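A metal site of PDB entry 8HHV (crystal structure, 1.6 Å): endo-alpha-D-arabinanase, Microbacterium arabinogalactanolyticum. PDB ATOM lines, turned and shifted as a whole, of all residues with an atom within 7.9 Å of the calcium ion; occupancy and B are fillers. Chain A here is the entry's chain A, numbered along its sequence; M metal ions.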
ATOM      1  N   ASP A 288       9.597  -4.522   0.639  1.00  0.00           N
ATOM      2  CA  ASP A 288       9.809  -3.089   0.631  1.00  0.00           C
ATOM      3  C   ASP A 288       9.157  -2.372   1.818  1.00  0.00           C
ATOM      4  O   ASP A 288       9.660  -1.326   2.229  1.00  0.00           O
ATOM      5  CB  ASP A 288       9.346  -2.449  -0.670  1.00  0.00           C
ATOM      6  CG  ASP A 288      10.214  -2.877  -1.827  1.00  0.00           C
ATOM      7  OD1 ASP A 288      11.457  -2.841  -1.674  1.00  0.00           O
ATOM      8  OD2 ASP A 288       9.626  -3.294  -2.768  1.00  0.00           O
ATOM      9  N   TYR A 289       8.004  -2.901   2.297  1.00  0.00           N
ATOM     10  CA  TYR A 289       7.166  -2.275   3.333  1.00  0.00           C
ATOM     11  C   TYR A 289       6.841  -3.345   4.364  1.00  0.00           C
ATOM     12  O   TYR A 289       5.734  -3.856   4.437  1.00  0.00           O
ATOM     13  CB  TYR A 289       5.942  -1.563   2.730  1.00  0.00           C
ATOM     14  CG  TYR A 289       6.420  -0.416   1.871  1.00  0.00           C
ATOM     15  CD1 TYR A 289       6.834   0.768   2.521  1.00  0.00           C
ATOM     16  CD2 TYR A 289       6.651  -0.527   0.500  1.00  0.00           C
ATOM     17  CE1 TYR A 289       7.449   1.783   1.797  1.00  0.00           C
ATOM     18  CE2 TYR A 289       7.263   0.504  -0.232  1.00  0.00           C
ATOM     19  CZ  TYR A 289       7.727   1.645   0.453  1.00  0.00           C
ATOM     20  OH  TYR A 289       8.401   2.659  -0.247  1.00  0.00           O
ATOM     21  N   PRO A 290       7.819  -3.667   5.260  1.00  0.00           N
ATOM     22  CA  PRO A 290       7.616  -4.802   6.171  1.00  0.00           C
ATOM     23  C   PRO A 290       6.461  -4.496   7.124  1.00  0.00           C
ATOM     24  O   PRO A 290       6.322  -3.360   7.593  1.00  0.00           O
ATOM     25  CB  PRO A 290       8.935  -4.881   6.963  1.00  0.00           C
ATOM     26  CG  PRO A 290       9.793  -3.720   6.535  1.00  0.00           C
ATOM     27  CD  PRO A 290       9.218  -3.192   5.242  1.00  0.00           C
ATOM     28  N   GLN A 312       1.618   0.605   8.840  1.00  0.00           N
ATOM     29  CA  GLN A 312       2.820  -0.232   9.021  1.00  0.00           C
ATOM     30  C   GLN A 312       3.085  -0.382  10.525  1.00  0.00           C
ATOM     31  O   GLN A 312       3.094   0.597  11.229  1.00  0.00           O
ATOM     32  CB  GLN A 312       3.963   0.389   8.201  1.00  0.00           C
ATOM     33  CG  GLN A 312       5.268  -0.416   8.213  1.00  0.00           C
ATOM     34  CD  GLN A 312       6.359   0.203   7.375  1.00  0.00           C
ATOM     35  OE1 GLN A 312       6.694   1.368   7.615  1.00  0.00           O
ATOM     36  NE2 GLN A 312       7.033  -0.615   6.563  1.00  0.00           N
ATOM     37  N   ASP A 339      14.708  -0.924  -4.768  1.00  0.00           N
ATOM     38  CA  ASP A 339      14.939  -0.912  -3.345  1.00  0.00           C
ATOM     39  C   ASP A 339      14.684   0.500  -2.799  1.00  0.00           C
ATOM     40  O   ASP A 339      15.516   1.002  -2.074  1.00  0.00           O
ATOM     41  CB  ASP A 339      16.365  -1.292  -2.965  1.00  0.00           C
ATOM     42  CG  ASP A 339      16.589  -1.619  -1.515  1.00  0.00           C
ATOM     43  OD1 ASP A 339      15.590  -1.834  -0.793  1.00  0.00           O
ATOM     44  OD2 ASP A 339      17.762  -1.693  -1.136  1.00  0.00           O
ATOM     45  N   ALA A 340      13.536   1.083  -3.159  1.00  0.00           N
ATOM     46  CA  ALA A 340      13.219   2.477  -2.845  1.00  0.00           C
ATOM     47  C   ALA A 340      13.258   2.825  -1.350  1.00  0.00           C
ATOM     48  O   ALA A 340      13.482   3.985  -1.008  1.00  0.00           O
ATOM     49  CB  ALA A 340      11.867   2.827  -3.368  1.00  0.00           C
ATOM     50  N   SER A 341      12.946   1.880  -0.454  1.00  0.00           N
ATOM     51  CA  SER A 341      12.879   2.152   0.986  1.00  0.00           C
ATOM     52  C   SER A 341      14.129   1.573   1.680  1.00  0.00           C
ATOM     53  O   SER A 341      14.152   1.407   2.863  1.00  0.00           O
ATOM     54  CB  SER A 341      11.565   1.565   1.520  1.00  0.00           C
ATOM     55  OG  SER A 341      11.234   2.086   2.779  1.00  0.00           O
ATOM     56  N   PHE A 342      15.160   1.170   0.926  1.00  0.00           N
ATOM     57  CA  PHE A 342      16.424   0.620   1.412  1.00  0.00           C
ATOM     58  C   PHE A 342      16.274  -0.681   2.211  1.00  0.00           C
ATOM     59  O   PHE A 342      17.237  -1.117   2.846  1.00  0.00           O
ATOM     60  CB  PHE A 342      17.189   1.706   2.147  1.00  0.00           C
ATOM     61  CG  PHE A 342      17.495   2.899   1.321  1.00  0.00           C
ATOM     62  CD1 PHE A 342      18.614   2.890   0.470  1.00  0.00           C
ATOM     63  CD2 PHE A 342      16.704   4.039   1.373  1.00  0.00           C
ATOM     64  CE1 PHE A 342      18.928   3.997  -0.266  1.00  0.00           C
ATOM     65  CE2 PHE A 342      16.994   5.147   0.616  1.00  0.00           C
ATOM     66  CZ  PHE A 342      18.100   5.138  -0.217  1.00  0.00           C
ATOM     67  N   GLU A 343      15.085  -1.320   2.204  1.00  0.00           N
ATOM     68  CA  GLU A 343      14.845  -2.448   3.100  1.00  0.00           C
ATOM     69  C   GLU A 343      15.489  -3.767   2.611  1.00  0.00           C
ATOM     70  O   GLU A 343      15.539  -4.748   3.386  1.00  0.00           O
ATOM     71  CB  GLU A 343      13.343  -2.713   3.270  1.00  0.00           C
ATOM     72  CG  GLU A 343      12.532  -1.528   3.762  1.00  0.00           C
ATOM     73  CD  GLU A 343      12.845  -1.062   5.163  1.00  0.00           C
ATOM     74  OE1 GLU A 343      12.912  -1.932   6.066  1.00  0.00           O
ATOM     75  OE2 GLU A 343      12.921   0.188   5.365  1.00  0.00           O
ATOM     76  N   ARG A 344      15.886  -3.794   1.340  1.00  0.00           N
ATOM     77  CA  ARG A 344      16.297  -5.048   0.691  1.00  0.00           C
ATOM     78  C   ARG A 344      17.773  -5.354   0.984  1.00  0.00           C
ATOM     79  O   ARG A 344      18.241  -6.511   0.728  1.00  0.00           O
ATOM     80  CB  ARG A 344      16.117  -4.986  -0.819  1.00  0.00           C
ATOM     81  CG  ARG A 344      14.688  -5.128  -1.295  1.00  0.00           C
ATOM     82  CD  ARG A 344      14.389  -4.871  -2.767  1.00  0.00           C
ATOM     83  NE  ARG A 344      12.934  -4.937  -2.998  1.00  0.00           N
ATOM     84  CZ  ARG A 344      12.243  -5.939  -3.554  1.00  0.00           C
ATOM     85  NH1 ARG A 344      12.791  -7.150  -3.754  1.00  0.00           N
ATOM     86  NH2 ARG A 344      10.954  -5.785  -3.797  1.00  0.00           N
ATOM     87  N   ILE A 364      23.456   1.780   5.507  1.00  0.00           N
ATOM     88  CA  ILE A 364      22.059   1.538   5.742  1.00  0.00           C
ATOM     89  C   ILE A 364      21.799   1.331   7.221  1.00  0.00           C
ATOM     90  O   ILE A 364      22.175   0.284   7.765  1.00  0.00           O
ATOM     91  CB  ILE A 364      21.586   0.325   4.901  1.00  0.00           C
ATOM     92  CG1 ILE A 364      21.953   0.425   3.412  1.00  0.00           C
ATOM     93  CG2 ILE A 364      20.099   0.065   5.163  1.00  0.00           C
ATOM     94  CD1 ILE A 364      21.519   1.709   2.675  1.00  0.00           C
ATOM     95  N   ASP A 365      21.231   2.365   7.905  1.00  0.00           N
ATOM     96  CA  ASP A 365      20.770   2.221   9.267  1.00  0.00           C
ATOM     97  C   ASP A 365      19.654   1.178   9.321  1.00  0.00           C
ATOM     98  O   ASP A 365      18.750   1.181   8.477  1.00  0.00           O
ATOM     99  CB  ASP A 365      20.273   3.559   9.828  1.00  0.00           C
ATOM    100  CG  ASP A 365      21.341   4.607  10.104  1.00  0.00           C
ATOM    101  OD1 ASP A 365      22.498   4.221  10.502  1.00  0.00           O
ATOM    102  OD2 ASP A 365      21.037   5.847   9.966  1.00  0.00           O
ATOM    103  N   ALA A 370      13.550   2.518  12.255  1.00  0.00           N
ATOM    104  CA  ALA A 370      14.551   3.534  11.946  1.00  0.00           C
ATOM    105  C   ALA A 370      14.224   4.251  10.637  1.00  0.00           C
ATOM    106  O   ALA A 370      14.636   5.394  10.459  1.00  0.00           O
ATOM    107  CB  ALA A 370      15.916   2.885  11.810  1.00  0.00           C
ATOM    108  N   GLY A 371      13.507   3.615   9.728  1.00  0.00           N
ATOM    109  CA  GLY A 371      13.259   4.242   8.439  1.00  0.00           C
ATOM    110  C   GLY A 371      12.212   5.337   8.616  1.00  0.00           C
ATOM    111  O   GLY A 371      11.478   5.422   9.613  1.00  0.00           O
ATOM    112  N   PHE A 372      12.109   6.161   7.592  1.00  0.00           N
ATOM    113  CA  PHE A 372      10.888   6.941   7.389  1.00  0.00           C
ATOM    114  C   PHE A 372       9.705   6.032   7.448  1.00  0.00           C
ATOM    115  O   PHE A 372       8.717   6.264   8.138  1.00  0.00           O
ATOM    116  CB  PHE A 372      10.967   7.761   6.100  1.00  0.00           C
ATOM    117  CG  PHE A 372       9.724   8.611   5.875  1.00  0.00           C
ATOM    118  CD1 PHE A 372       9.370   9.621   6.770  1.00  0.00           C
ATOM    119  CD2 PHE A 372       8.860   8.351   4.850  1.00  0.00           C
ATOM    120  CE1 PHE A 372       8.222  10.365   6.553  1.00  0.00           C
ATOM    121  CE2 PHE A 372       7.718   9.099   4.626  1.00  0.00           C
ATOM    122  CZ  PHE A 372       7.391  10.092   5.491  1.00  0.00           C
ATOM    123  N   THR A 373       9.781   4.967   6.576  1.00  0.00           N
ATOM    124  CA  THR A 373       9.012   3.763   6.703  1.00  0.00           C
ATOM    125  C   THR A 373      10.006   2.617   6.907  1.00  0.00           C
ATOM    126  O   THR A 373      11.110   2.696   6.364  1.00  0.00           O
ATOM    127  CB  THR A 373       8.132   3.510   5.445  1.00  0.00           C
ATOM    128  OG1 THR A 373       9.001   3.291   4.327  1.00  0.00           O
ATOM    129  CG2 THR A 373       7.185   4.640   5.110  1.00  0.00           C
ATOM    130  N   GLY A 374       9.513   1.562   7.526  1.00  0.00           N
ATOM    131  CA  GLY A 374      10.210   0.285   7.646  1.00  0.00           C
ATOM    132  C   GLY A 374      11.406   0.488   8.584  1.00  0.00           C
ATOM    133  O   GLY A 374      11.438   1.401   9.403  1.00  0.00           O
ATOM    134  N   ASP A 375      12.358  -0.437   8.527  1.00  0.00           N
ATOM    135  CA  ASP A 375      13.439  -0.468   9.486  1.00  0.00           C
ATOM    136  C   ASP A 375      14.762   0.019   8.885  1.00  0.00           C
ATOM    137  O   ASP A 375      15.771   0.075   9.592  1.00  0.00           O
ATOM    138  CB  ASP A 375      13.616  -1.923   9.987  1.00  0.00           C
ATOM    139  CG  ASP A 375      12.583  -2.376  10.979  1.00  0.00           C
ATOM    140  OD1 ASP A 375      11.660  -1.600  11.374  1.00  0.00           O
ATOM    141  OD2 ASP A 375      12.796  -3.485  11.485  1.00  0.00           O
ATOM    142  N   HIS A 376      14.777   0.415   7.607  1.00  0.00           N
ATOM    143  CA  HIS A 376      16.031   0.828   6.972  1.00  0.00           C
ATOM    144  C   HIS A 376      15.836   2.223   6.374  1.00  0.00           C
ATOM    145  O   HIS A 376      14.752   2.571   5.886  1.00  0.00           O
ATOM    146  CB  HIS A 376      16.361  -0.113   5.800  1.00  0.00           C
ATOM    147  CG  HIS A 376      16.785  -1.495   6.185  1.00  0.00           C
ATOM    148  ND1 HIS A 376      17.521  -2.263   5.311  1.00  0.00           N
ATOM    149  CD2 HIS A 376      16.594  -2.237   7.255  1.00  0.00           C
ATOM    150  CE1 HIS A 376      17.699  -3.466   5.817  1.00  0.00           C
ATOM    151  NE2 HIS A 376      17.220  -3.437   7.060  1.00  0.00           N
ATOM    152  N   ARG A 377      16.941   2.978   6.418  1.00  0.00           N
ATOM    153  CA  ARG A 377      17.152   4.256   5.721  1.00  0.00           C
ATOM    154  C   ARG A 377      18.637   4.286   5.318  1.00  0.00           C
ATOM    155  O   ARG A 377      19.419   3.576   5.918  1.00  0.00           O
ATOM    156  CB  ARG A 377      16.742   5.400   6.660  1.00  0.00           C
ATOM    157  CG  ARG A 377      17.606   5.469   7.895  1.00  0.00           C
ATOM    158  CD  ARG A 377      17.315   6.544   8.918  1.00  0.00           C
ATOM    159  NE  ARG A 377      18.299   6.571  10.031  1.00  0.00           N
ATOM    160  CZ  ARG A 377      17.990   6.556  11.298  1.00  0.00           C
ATOM    161  NH1 ARG A 377      16.718   6.667  11.728  1.00  0.00           N
ATOM    162  NH2 ARG A 377      18.957   6.555  12.200  1.00  0.00           N
ATOM    163  N   ALA A 378      18.967   5.155   4.393  1.00  0.00           N
ATOM    164  CA  ALA A 378      20.332   5.420   3.979  1.00  0.00           C
ATOM    165  C   ALA A 378      20.801   6.662   4.729  1.00  0.00           C
ATOM    166  O   ALA A 378      20.017   7.525   5.081  1.00  0.00           O
ATOM    167  CB  ALA A 378      20.455   5.557   2.495  1.00  0.00           C
ATOM    168  N   TRP A 439      11.793  14.659   9.038  1.00  0.00           N
ATOM    169  CA  TRP A 439      11.666  14.016   7.731  1.00  0.00           C
ATOM    170  C   TRP A 439      10.810  14.930   6.815  1.00  0.00           C
ATOM    171  O   TRP A 439       9.679  15.327   7.176  1.00  0.00           O
ATOM    172  CB  TRP A 439      11.061  12.632   7.855  1.00  0.00           C
ATOM    173  CG  TRP A 439      11.929  11.548   8.367  1.00  0.00           C
ATOM    174  CD1 TRP A 439      11.728  10.854   9.532  1.00  0.00           C
ATOM    175  CD2 TRP A 439      12.985  10.853   7.639  1.00  0.00           C
ATOM    176  NE1 TRP A 439      12.681   9.859   9.656  1.00  0.00           N
ATOM    177  CE2 TRP A 439      13.453   9.830   8.505  1.00  0.00           C
ATOM    178  CE3 TRP A 439      13.597  11.011   6.379  1.00  0.00           C
ATOM    179  CZ2 TRP A 439      14.451   8.925   8.116  1.00  0.00           C
ATOM    180  CZ3 TRP A 439      14.546  10.080   5.973  1.00  0.00           C
ATOM    181  CH2 TRP A 439      15.033   9.114   6.861  1.00  0.00           C
ATOM    182  N   LEU A 471      18.041   9.496   4.207  1.00  0.00           N
ATOM    183  CA  LEU A 471      17.224   9.419   3.009  1.00  0.00           C
ATOM    184  C   LEU A 471      16.379   8.113   2.989  1.00  0.00           C
ATOM    185  O   LEU A 471      16.864   7.025   3.371  1.00  0.00           O
ATOM    186  CB  LEU A 471      18.197   9.486   1.802  1.00  0.00           C
ATOM    187  CG  LEU A 471      17.577   9.374   0.393  1.00  0.00           C
ATOM    188  CD1 LEU A 471      16.774  10.606   0.089  1.00  0.00           C
ATOM    189  CD2 LEU A 471      18.697   9.204  -0.658  1.00  0.00           C
ATOM    190  N   ASP A 472      15.132   8.201   2.522  1.00  0.00           N
ATOM    191  CA  ASP A 472      14.254   7.042   2.426  1.00  0.00           C
ATOM    192  C   ASP A 472      13.148   7.269   1.370  1.00  0.00           C
ATOM    193  O   ASP A 472      12.806   8.452   1.089  1.00  0.00           O
ATOM    194  CB  ASP A 472      13.641   6.654   3.784  1.00  0.00           C
ATOM    195  CG  ASP A 472      13.294   5.187   4.005  1.00  0.00           C
ATOM    196  OD1 ASP A 472      13.442   4.308   3.074  1.00  0.00           O
ATOM    197  OD2 ASP A 472      12.753   4.876   5.133  1.00  0.00           O
ATOM    198  N   ASP A 473      12.629   6.189   0.835  1.00  0.00           N
ATOM    199  CA  ASP A 473      11.353   6.100   0.056  1.00  0.00           C
ATOM    200  C   ASP A 473      11.418   6.981  -1.180  1.00  0.00           C
ATOM    201  O   ASP A 473      10.536   7.787  -1.472  1.00  0.00           O
ATOM    202  CB  ASP A 473      10.175   6.347   1.011  1.00  0.00           C
ATOM    203  CG  ASP A 473       9.941   5.200   1.960  1.00  0.00           C
ATOM    204  OD1 ASP A 473       9.887   3.996   1.421  1.00  0.00           O
ATOM    205  OD2 ASP A 473       9.957   5.453   3.198  1.00  0.00           O
ATOM    206  N   VAL A 474      12.530   6.816  -1.922  1.00  0.00           N
ATOM    207  CA  VAL A 474      12.763   7.583  -3.132  1.00  0.00           C
ATOM    208  C   VAL A 474      11.986   6.956  -4.299  1.00  0.00           C
ATOM    209  O   VAL A 474      12.014   5.736  -4.506  1.00  0.00           O
ATOM    210  CB  VAL A 474      14.262   7.670  -3.413  1.00  0.00           C
ATOM    211  CG1 VAL A 474      14.545   8.496  -4.644  1.00  0.00           C
ATOM    212  CG2 VAL A 474      15.095   8.173  -2.210  1.00  0.00           C
HETATM  213 CA    CA M   1      12.785   2.456   4.620  1.00  0.00          CA
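O of Phe 342 lies within hydrogen-bond range of ND1 of His 376 (2.7 Å).
N of Asp 375 is in hydrogen-bond range of OE1 of Glu 343 (2.9 Å).
N of Glu 343 is in hydrogen-bond range of OD1 of Asp 339, at 3.1 Å.
OG1 of Thr 373 lies within hydrogen-bond range of OD2 of Asp 473 (2.6 Å).
OD1 of Asp 473 lies close to OG of Ser 341, 2.7 Å away.
OD2 of Asp 472 sits close to N of Phe 372 (2.8 Å).
Within 4 Å of the calcium ion: Ser 341, Glu 343, Thr 373, His 376 and Asp 472.
The nearest printed residue that does not touch the calcium ion is Gly 371 (4.2 Å).
O of His 376 binds the calcium ion (2.3 Å).
OE2 of Glu 343 is bound to the calcium ion, 2.4 Å away.
The calcium ion is bound by O of Thr 373 (2.4 Å).
OG of Ser 341 is bound to the calcium ion (2.4 Å).
O of Ser 341 binds the calcium ion, at 2.5 Å.
OD2 of Asp 472 binds the calcium ion (2.5 Å).
The calcium ion is bound by OD1 of Asp 472 (2.5 Å).
The calcium ion has seven donor atoms within binding distance.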
